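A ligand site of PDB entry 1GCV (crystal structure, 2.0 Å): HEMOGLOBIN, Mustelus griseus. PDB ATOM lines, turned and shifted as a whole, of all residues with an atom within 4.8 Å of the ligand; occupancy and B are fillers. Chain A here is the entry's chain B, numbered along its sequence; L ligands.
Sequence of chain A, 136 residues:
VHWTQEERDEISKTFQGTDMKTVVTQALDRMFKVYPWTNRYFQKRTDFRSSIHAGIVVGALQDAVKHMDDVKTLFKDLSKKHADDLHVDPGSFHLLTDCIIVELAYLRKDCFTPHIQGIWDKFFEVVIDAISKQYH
The side-chain sulfur (SD) of Met 31 lies close to the backbone NH (N) of Leu 96 (3.7 Å).
The backbone NH (N) of Val 88 lies within hydrogen-bond range of the backbone carbonyl oxygen (O) of His 82 (3.0 Å).
A ring nitrogen (ND1) of His 82 lies within hydrogen-bond range of the backbone carbonyl oxygen of Leu 78, at 2.7 Å.
N of Leu 86 is in hydrogen-bond range of O of Lys 81, 3.0 Å away.
An iron atom (FE1) of the ligand is bound by a ring nitrogen (NE2) of His 82.
The side-chain amino group (NZ) of Lys 81 is in salt-bridge range of an oxygen (O2) of the ligand, at 3.1 Å.
Merely in contact with the ligand: Thr 38 (3.96 Å), Tyr 41 (3.5 Å), Phe 42 (3.6 Å), Arg 45 (3.3 Å), His 53 (3.6 Å), Ile 56 (3.4 Å), Val 57 (3.998 Å), Ala 60 (3.8 Å), Leu 78 (3.5 Å), Leu 86 (3.4 Å), Val 88 (3.5 Å), Ser 92 (3.7 Å), Phe 93 (3.8 Å), Leu 96 (3.7 Å) and Ile 131 (3.8 Å).
Hydrophobic or aromatic side chains that line the ligand: Tyr 41, Phe 42, His 53, Ile 56, Val 57, Ala 60, Leu 78, His 82, Leu 86, Val 88, Phe 93, Leu 96 and Ile 131.
Within 4 Å of the ligand: Thr 38, Tyr 41, Phe 42, Arg 45, His 53, Ile 56, Val 57, Ala 60, Leu 78, Lys 81, His 82, Leu 86, Val 88, Ser 92, Phe 93, Leu 96 and Ile 131.
Along chain A the residues within 4 Å of the ligand span positions 38 to 131.
The nearest printed residue that does not touch the ligand is Thr 97 (4.05 Å).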
ATOM      1  N   MET A  31      24.905   9.526  10.084  1.00  0.00           N
ATOM      2  CA  MET A  31      23.698   8.743   9.833  1.00  0.00           C
ATOM      3  C   MET A  31      23.922   7.236   9.995  1.00  0.00           C
ATOM      4  O   MET A  31      23.066   6.550  10.564  1.00  0.00           O
ATOM      5  CB  MET A  31      23.170   9.029   8.427  1.00  0.00           C
ATOM      6  CG  MET A  31      21.859   8.321   8.117  1.00  0.00           C
ATOM      7  SD  MET A  31      21.335   8.537   6.411  1.00  0.00           S
ATOM      8  CE  MET A  31      22.534   7.540   5.560  1.00  0.00           C
ATOM      9  N   THR A  38      20.364   2.187   8.063  1.00  0.00           N
ATOM     10  CA  THR A  38      20.559   2.825   6.758  1.00  0.00           C
ATOM     11  C   THR A  38      21.787   2.274   6.032  1.00  0.00           C
ATOM     12  O   THR A  38      22.003   2.580   4.867  1.00  0.00           O
ATOM     13  CB  THR A  38      20.706   4.369   6.868  1.00  0.00           C
ATOM     14  OG1 THR A  38      21.832   4.676   7.694  1.00  0.00           O
ATOM     15  CG2 THR A  38      19.454   4.994   7.456  1.00  0.00           C
ATOM     16  N   TYR A  41      21.721  -0.325   2.499  1.00  0.00           N
ATOM     17  CA  TYR A  41      21.967  -0.041   1.081  1.00  0.00           C
ATOM     18  C   TYR A  41      23.420  -0.011   0.610  1.00  0.00           C
ATOM     19  O   TYR A  41      23.675  -0.201  -0.579  1.00  0.00           O
ATOM     20  CB  TYR A  41      21.300   1.293   0.707  1.00  0.00           C
ATOM     21  CG  TYR A  41      19.886   1.428   1.246  1.00  0.00           C
ATOM     22  CD1 TYR A  41      18.819   0.799   0.608  1.00  0.00           C
ATOM     23  CD2 TYR A  41      19.630   2.125   2.426  1.00  0.00           C
ATOM     24  CE1 TYR A  41      17.541   0.852   1.126  1.00  0.00           C
ATOM     25  CE2 TYR A  41      18.345   2.202   2.957  1.00  0.00           C
ATOM     26  CZ  TYR A  41      17.313   1.557   2.305  1.00  0.00           C
ATOM     27  OH  TYR A  41      16.038   1.598   2.817  1.00  0.00           O
ATOM     28  N   PHE A  42      24.359   0.199   1.519  1.00  0.00           N
ATOM     29  CA  PHE A  42      25.771   0.294   1.137  1.00  0.00           C
ATOM     30  C   PHE A  42      26.680  -0.860   1.535  1.00  0.00           C
ATOM     31  O   PHE A  42      27.753  -1.023   0.958  1.00  0.00           O
ATOM     32  CB  PHE A  42      26.343   1.612   1.669  1.00  0.00           C
ATOM     33  CG  PHE A  42      25.484   2.807   1.364  1.00  0.00           C
ATOM     34  CD1 PHE A  42      24.693   3.371   2.348  1.00  0.00           C
ATOM     35  CD2 PHE A  42      25.443   3.341   0.081  1.00  0.00           C
ATOM     36  CE1 PHE A  42      23.866   4.455   2.066  1.00  0.00           C
ATOM     37  CE2 PHE A  42      24.625   4.424  -0.211  1.00  0.00           C
ATOM     38  CZ  PHE A  42      23.839   4.973   0.790  1.00  0.00           C
ATOM     39  N   ARG A  45      27.748  -2.502  -1.601  1.00  0.00           N
ATOM     40  CA  ARG A  45      28.665  -1.873  -2.544  1.00  0.00           C
ATOM     41  C   ARG A  45      30.013  -1.864  -1.860  1.00  0.00           C
ATOM     42  O   ARG A  45      30.282  -1.008  -1.024  1.00  0.00           O
ATOM     43  CB  ARG A  45      28.227  -0.448  -2.855  1.00  0.00           C
ATOM     44  CG  ARG A  45      26.731  -0.204  -2.738  1.00  0.00           C
ATOM     45  CD  ARG A  45      26.270   0.819  -3.770  1.00  0.00           C
ATOM     46  NE  ARG A  45      24.810   0.851  -3.888  1.00  0.00           N
ATOM     47  CZ  ARG A  45      24.104   0.007  -4.627  1.00  0.00           C
ATOM     48  NH1 ARG A  45      24.719  -0.943  -5.321  1.00  0.00           N
ATOM     49  NH2 ARG A  45      22.786   0.125  -4.690  1.00  0.00           N
ATOM     50  N   HIS A  53      30.046   9.629  -2.450  1.00  0.00           N
ATOM     51  CA  HIS A  53      28.592   9.661  -2.378  1.00  0.00           C
ATOM     52  C   HIS A  53      28.091  11.059  -2.000  1.00  0.00           C
ATOM     53  O   HIS A  53      27.159  11.582  -2.608  1.00  0.00           O
ATOM     54  CB  HIS A  53      28.098   8.637  -1.348  1.00  0.00           C
ATOM     55  CG  HIS A  53      26.638   8.391  -1.675  1.00  0.00           C
ATOM     56  ND1 HIS A  53      26.208   8.025  -2.950  1.00  0.00           N
ATOM     57  CD2 HIS A  53      25.598   8.563  -0.770  1.00  0.00           C
ATOM     58  CE1 HIS A  53      24.885   7.981  -2.803  1.00  0.00           C
ATOM     59  NE2 HIS A  53      24.499   8.281  -1.599  1.00  0.00           N
ATOM     60  N   ILE A  56      28.086  13.283  -4.837  1.00  0.00           N
ATOM     61  CA  ILE A  56      26.980  12.991  -5.745  1.00  0.00           C
ATOM     62  C   ILE A  56      25.658  13.547  -5.187  1.00  0.00           C
ATOM     63  O   ILE A  56      24.801  14.001  -5.950  1.00  0.00           O
ATOM     64  CB  ILE A  56      26.847  11.459  -5.962  1.00  0.00           C
ATOM     65  CG1 ILE A  56      27.916  10.987  -6.956  1.00  0.00           C
ATOM     66  CG2 ILE A  56      25.475  11.120  -6.503  1.00  0.00           C
ATOM     67  CD1 ILE A  56      28.436   9.594  -6.692  1.00  0.00           C
ATOM     68  N   VAL A  57      25.516  13.518  -3.869  1.00  0.00           N
ATOM     69  CA  VAL A  57      24.300  14.018  -3.241  1.00  0.00           C
ATOM     70  C   VAL A  57      24.267  15.554  -3.277  1.00  0.00           C
ATOM     71  O   VAL A  57      23.231  16.154  -3.554  1.00  0.00           O
ATOM     72  CB  VAL A  57      24.206  13.526  -1.784  1.00  0.00           C
ATOM     73  CG1 VAL A  57      23.094  14.262  -1.033  1.00  0.00           C
ATOM     74  CG2 VAL A  57      23.952  12.027  -1.771  1.00  0.00           C
ATOM     75  N   ALA A  60      23.238  17.101  -6.513  1.00  0.00           N
ATOM     76  CA  ALA A  60      21.793  17.091  -6.747  1.00  0.00           C
ATOM     77  C   ALA A  60      21.143  18.235  -5.971  1.00  0.00           C
ATOM     78  O   ALA A  60      20.272  18.934  -6.487  1.00  0.00           O
ATOM     79  CB  ALA A  60      21.187  15.755  -6.297  1.00  0.00           C
ATOM     80  N   LEU A  61      21.569  18.427  -4.728  1.00  0.00           N
ATOM     81  CA  LEU A  61      21.039  19.502  -3.898  1.00  0.00           C
ATOM     82  C   LEU A  61      21.377  20.852  -4.534  1.00  0.00           C
ATOM     83  O   LEU A  61      20.545  21.748  -4.574  1.00  0.00           O
ATOM     84  CB  LEU A  61      21.640  19.434  -2.490  1.00  0.00           C
ATOM     85  CG  LEU A  61      21.179  18.252  -1.628  1.00  0.00           C
ATOM     86  CD1 LEU A  61      21.861  18.291  -0.271  1.00  0.00           C
ATOM     87  CD2 LEU A  61      19.658  18.314  -1.493  1.00  0.00           C
ATOM     88  N   PHE A  75      13.587  16.488  -9.842  1.00  0.00           N
ATOM     89  CA  PHE A  75      13.936  15.219  -9.188  1.00  0.00           C
ATOM     90  C   PHE A  75      13.054  14.040  -9.606  1.00  0.00           C
ATOM     91  O   PHE A  75      13.128  12.971  -8.994  1.00  0.00           O
ATOM     92  CB  PHE A  75      13.856  15.376  -7.654  1.00  0.00           C
ATOM     93  CG  PHE A  75      15.091  15.970  -7.015  1.00  0.00           C
ATOM     94  CD1 PHE A  75      15.177  16.090  -5.634  1.00  0.00           C
ATOM     95  CD2 PHE A  75      16.162  16.420  -7.785  1.00  0.00           C
ATOM     96  CE1 PHE A  75      16.309  16.640  -5.029  1.00  0.00           C
ATOM     97  CE2 PHE A  75      17.299  16.962  -7.195  1.00  0.00           C
ATOM     98  CZ  PHE A  75      17.370  17.076  -5.810  1.00  0.00           C
ATOM     99  N   LEU A  78      15.325  11.107 -10.520  1.00  0.00           N
ATOM    100  CA  LEU A  78      16.101  10.724  -9.344  1.00  0.00           C
ATOM    101  C   LEU A  78      15.192   9.968  -8.391  1.00  0.00           C
ATOM    102  O   LEU A  78      15.595   8.989  -7.756  1.00  0.00           O
ATOM    103  CB  LEU A  78      16.657  11.974  -8.643  1.00  0.00           C
ATOM    104  CG  LEU A  78      17.575  11.761  -7.446  1.00  0.00           C
ATOM    105  CD1 LEU A  78      18.695  10.852  -7.850  1.00  0.00           C
ATOM    106  CD2 LEU A  78      18.114  13.099  -6.968  1.00  0.00           C
ATOM    107  N   LYS A  81      14.503   6.533  -9.728  1.00  0.00           N
ATOM    108  CA  LYS A  81      15.724   5.744  -9.571  1.00  0.00           C
ATOM    109  C   LYS A  81      15.820   5.186  -8.151  1.00  0.00           C
ATOM    110  O   LYS A  81      16.249   4.051  -7.955  1.00  0.00           O
ATOM    111  CB  LYS A  81      16.947   6.619  -9.875  1.00  0.00           C
ATOM    112  CG  LYS A  81      18.268   5.989  -9.465  1.00  0.00           C
ATOM    113  CD  LYS A  81      19.077   5.533 -10.676  1.00  0.00           C
ATOM    114  CE  LYS A  81      19.840   4.248 -10.407  1.00  0.00           C
ATOM    115  NZ  LYS A  81      21.223   4.493  -9.884  1.00  0.00           N
ATOM    116  N   HIS A  82      15.423   5.970  -7.148  1.00  0.00           N
ATOM    117  CA  HIS A  82      15.477   5.508  -5.761  1.00  0.00           C
ATOM    118  C   HIS A  82      14.384   4.496  -5.454  1.00  0.00           C
ATOM    119  O   HIS A  82      14.595   3.554  -4.682  1.00  0.00           O
ATOM    120  CB  HIS A  82      15.338   6.689  -4.792  1.00  0.00           C
ATOM    121  CG  HIS A  82      16.600   7.478  -4.586  1.00  0.00           C
ATOM    122  ND1 HIS A  82      17.019   8.352  -5.590  1.00  0.00           N
ATOM    123  CD2 HIS A  82      17.488   7.405  -3.512  1.00  0.00           C
ATOM    124  CE1 HIS A  82      18.200   8.762  -5.116  1.00  0.00           C
ATOM    125  NE2 HIS A  82      18.507   8.270  -3.956  1.00  0.00           N
ATOM    126  N   LEU A  86      17.110   1.452  -6.801  1.00  0.00           N
ATOM    127  CA  LEU A  86      17.778   1.275  -5.526  1.00  0.00           C
ATOM    128  C   LEU A  86      16.932   0.712  -4.390  1.00  0.00           C
ATOM    129  O   LEU A  86      17.458   0.166  -3.430  1.00  0.00           O
ATOM    130  CB  LEU A  86      18.374   2.619  -5.092  1.00  0.00           C
ATOM    131  CG  LEU A  86      19.196   3.275  -6.214  1.00  0.00           C
ATOM    132  CD1 LEU A  86      19.331   4.768  -5.984  1.00  0.00           C
ATOM    133  CD2 LEU A  86      20.560   2.617  -6.259  1.00  0.00           C
ATOM    134  N   VAL A  88      15.217   2.270  -2.054  1.00  0.00           N
ATOM    135  CA  VAL A  88      15.530   2.958  -0.813  1.00  0.00           C
ATOM    136  C   VAL A  88      14.199   3.293  -0.140  1.00  0.00           C
ATOM    137  O   VAL A  88      13.294   3.829  -0.771  1.00  0.00           O
ATOM    138  CB  VAL A  88      16.329   4.269  -1.064  1.00  0.00           C
ATOM    139  CG1 VAL A  88      16.532   5.030   0.245  1.00  0.00           C
ATOM    140  CG2 VAL A  88      17.669   3.935  -1.687  1.00  0.00           C
ATOM    141  N   SER A  92      13.662   6.813   5.117  1.00  0.00           N
ATOM    142  CA  SER A  92      15.051   7.024   5.503  1.00  0.00           C
ATOM    143  C   SER A  92      15.617   8.348   4.992  1.00  0.00           C
ATOM    144  O   SER A  92      16.663   8.789   5.457  1.00  0.00           O
ATOM    145  CB  SER A  92      15.908   5.859   5.003  1.00  0.00           C
ATOM    146  OG  SER A  92      15.485   4.649   5.610  1.00  0.00           O
ATOM    147  N   PHE A  93      14.930   8.977   4.037  1.00  0.00           N
ATOM    148  CA  PHE A  93      15.394  10.243   3.470  1.00  0.00           C
ATOM    149  C   PHE A  93      15.637  11.333   4.521  1.00  0.00           C
ATOM    150  O   PHE A  93      16.662  12.005   4.494  1.00  0.00           O
ATOM    151  CB  PHE A  93      14.410  10.758   2.414  1.00  0.00           C
ATOM    152  CG  PHE A  93      14.451   9.989   1.113  1.00  0.00           C
ATOM    153  CD1 PHE A  93      15.664   9.607   0.542  1.00  0.00           C
ATOM    154  CD2 PHE A  93      13.280   9.640   0.466  1.00  0.00           C
ATOM    155  CE1 PHE A  93      15.697   8.896  -0.655  1.00  0.00           C
ATOM    156  CE2 PHE A  93      13.309   8.922  -0.737  1.00  0.00           C
ATOM    157  CZ  PHE A  93      14.521   8.555  -1.287  1.00  0.00           C
ATOM    158  N   LEU A  96      18.925  11.379   6.704  1.00  0.00           N
ATOM    159  CA  LEU A  96      20.116  12.009   6.157  1.00  0.00           C
ATOM    160  C   LEU A  96      20.014  13.525   6.295  1.00  0.00           C
ATOM    161  O   LEU A  96      20.916  14.159   6.833  1.00  0.00           O
ATOM    162  CB  LEU A  96      20.305  11.649   4.678  1.00  0.00           C
ATOM    163  CG  LEU A  96      21.401  12.445   3.939  1.00  0.00           C
ATOM    164  CD1 LEU A  96      22.739  12.223   4.615  1.00  0.00           C
ATOM    165  CD2 LEU A  96      21.461  11.998   2.490  1.00  0.00           C
ATOM    166  N   THR A  97      18.905  14.107   5.840  1.00  0.00           N
ATOM    167  CA  THR A  97      18.728  15.553   5.911  1.00  0.00           C
ATOM    168  C   THR A  97      18.765  16.040   7.367  1.00  0.00           C
ATOM    169  O   THR A  97      19.254  17.131   7.644  1.00  0.00           O
ATOM    170  CB  THR A  97      17.422  16.031   5.203  1.00  0.00           C
ATOM    171  OG1 THR A  97      16.282  15.412   5.802  1.00  0.00           O
ATOM    172  CG2 THR A  97      17.468  15.663   3.739  1.00  0.00           C
ATOM    173  N   VAL A 127      12.712  18.972  -0.450  1.00  0.00           N
ATOM    174  CA  VAL A 127      13.565  18.005  -1.141  1.00  0.00           C
ATOM    175  C   VAL A 127      13.124  16.542  -0.874  1.00  0.00           C
ATOM    176  O   VAL A 127      13.146  15.718  -1.787  1.00  0.00           O
ATOM    177  CB  VAL A 127      15.052  18.217  -0.734  1.00  0.00           C
ATOM    178  CG1 VAL A 127      15.862  16.971  -0.997  1.00  0.00           C
ATOM    179  CG2 VAL A 127      15.627  19.391  -1.520  1.00  0.00           C
ATOM    180  N   ILE A 128      12.703  16.251   0.353  1.00  0.00           N
ATOM    181  CA  ILE A 128      12.230  14.902   0.728  1.00  0.00           C
ATOM    182  C   ILE A 128      10.962  14.584  -0.062  1.00  0.00           C
ATOM    183  O   ILE A 128      10.779  13.470  -0.551  1.00  0.00           O
ATOM    184  CB  ILE A 128      11.888  14.806   2.238  1.00  0.00           C
ATOM    185  CG1 ILE A 128      13.114  15.075   3.097  1.00  0.00           C
ATOM    186  CG2 ILE A 128      11.303  13.444   2.547  1.00  0.00           C
ATOM    187  CD1 ILE A 128      14.235  14.089   2.918  1.00  0.00           C
ATOM    188  N   ILE A 131      11.758  13.968  -3.850  1.00  0.00           N
ATOM    189  CA  ILE A 131      12.408  12.681  -4.075  1.00  0.00           C
ATOM    190  C   ILE A 131      11.576  11.465  -3.647  1.00  0.00           C
ATOM    191  O   ILE A 131      11.912  10.335  -3.995  1.00  0.00           O
ATOM    192  CB  ILE A 131      13.809  12.656  -3.377  1.00  0.00           C
ATOM    193  CG1 ILE A 131      14.728  11.674  -4.111  1.00  0.00           C
ATOM    194  CG2 ILE A 131      13.656  12.300  -1.912  1.00  0.00           C
ATOM    195  CD1 ILE A 131      16.187  11.797  -3.692  1.00  0.00           C
HETATM  196  C1  LIG L   1      22.289   7.329  -5.462  1.00  0.00           C
HETATM  197  C2  LIG L   1      20.726  11.818  -4.437  1.00  0.00           C
HETATM  198  C3  LIG L   1      19.328  10.264  -0.040  1.00  0.00           C
HETATM  199  C4  LIG L   1      20.799   5.772  -1.108  1.00  0.00           C
HETATM  200  C5  LIG L   1      21.998   8.700  -5.528  1.00  0.00           C
HETATM  201  C6  LIG L   1      22.344   9.559  -6.638  1.00  0.00           C
HETATM  202  C7  LIG L   1      21.915  10.806  -6.358  1.00  0.00           C
HETATM  203  C8  LIG L   1      21.308  10.733  -5.051  1.00  0.00           C
HETATM  204  C9  LIG L   1      21.972  12.030  -7.252  1.00  0.00           C
HETATM  205  C10 LIG L   1      23.076   9.182  -7.901  1.00  0.00           C
HETATM  206  C11 LIG L   1      22.049   8.735  -8.907  1.00  0.00           C
HETATM  207  C12 LIG L   1      22.621   7.797  -9.930  1.00  0.00           C
HETATM  208  O1  LIG L   1      22.449   8.057 -11.140  1.00  0.00           O
HETATM  209  O2  LIG L   1      23.251   6.789  -9.538  1.00  0.00           O
HETATM  210  C13 LIG L   1      20.148  11.770  -3.193  1.00  0.00           C
HETATM  211  C14 LIG L   1      19.629  12.949  -2.535  1.00  0.00           C
HETATM  212  C15 LIG L   1      19.290  12.544  -1.252  1.00  0.00           C
HETATM  213  C16 LIG L   1      19.539  11.083  -1.177  1.00  0.00           C
HETATM  214  C17 LIG L   1      19.469  14.332  -3.179  1.00  0.00           C
HETATM  215  C18 LIG L   1      18.869  13.399  -0.224  1.00  0.00           C
HETATM  216  C19 LIG L   1      17.693  13.210   0.525  1.00  0.00           C
HETATM  217  C20 LIG L   1      19.578   8.880   0.046  1.00  0.00           C
HETATM  218  C21 LIG L   1      19.437   8.079   1.265  1.00  0.00           C
HETATM  219  C22 LIG L   1      19.777   6.798   0.924  1.00  0.00           C
HETATM  220  C23 LIG L   1      20.213   6.842  -0.469  1.00  0.00           C
HETATM  221  C24 LIG L   1      19.073   8.559   2.673  1.00  0.00           C
HETATM  222  C25 LIG L   1      19.661   5.628   1.685  1.00  0.00           C
HETATM  223  C26 LIG L   1      20.060   5.496   3.027  1.00  0.00           C
HETATM  224  C27 LIG L   1      21.295   5.812  -2.397  1.00  0.00           C
HETATM  225  C28 LIG L   1      21.963   4.695  -3.013  1.00  0.00           C
HETATM  226  C29 LIG L   1      22.415   5.128  -4.210  1.00  0.00           C
HETATM  227  C30 LIG L   1      21.964   6.511  -4.371  1.00  0.00           C
HETATM  228  C31 LIG L   1      22.068   3.279  -2.446  1.00  0.00           C
HETATM  229  C32 LIG L   1      23.262   4.346  -5.206  1.00  0.00           C
HETATM  230  C33 LIG L   1      24.641   4.045  -4.638  1.00  0.00           C
HETATM  231  C34 LIG L   1      25.726   4.064  -5.693  1.00  0.00           C
HETATM  232  O3  LIG L   1      26.897   4.268  -5.318  1.00  0.00           O
HETATM  233  O4  LIG L   1      25.405   3.878  -6.889  1.00  0.00           O
HETATM  234  N1  LIG L   1      21.321   9.416  -4.550  1.00  0.00           N
HETATM  235  N2  LIG L   1      20.059  10.615  -2.382  1.00  0.00           N
HETATM  236  N3  LIG L   1      20.052   8.108  -1.030  1.00  0.00           N
HETATM  237  N4  LIG L   1      21.279   6.918  -3.234  1.00  0.00           N
HETATM  238 FE1  LIG L   1      20.433   8.712  -2.904  1.00  0.00          FE
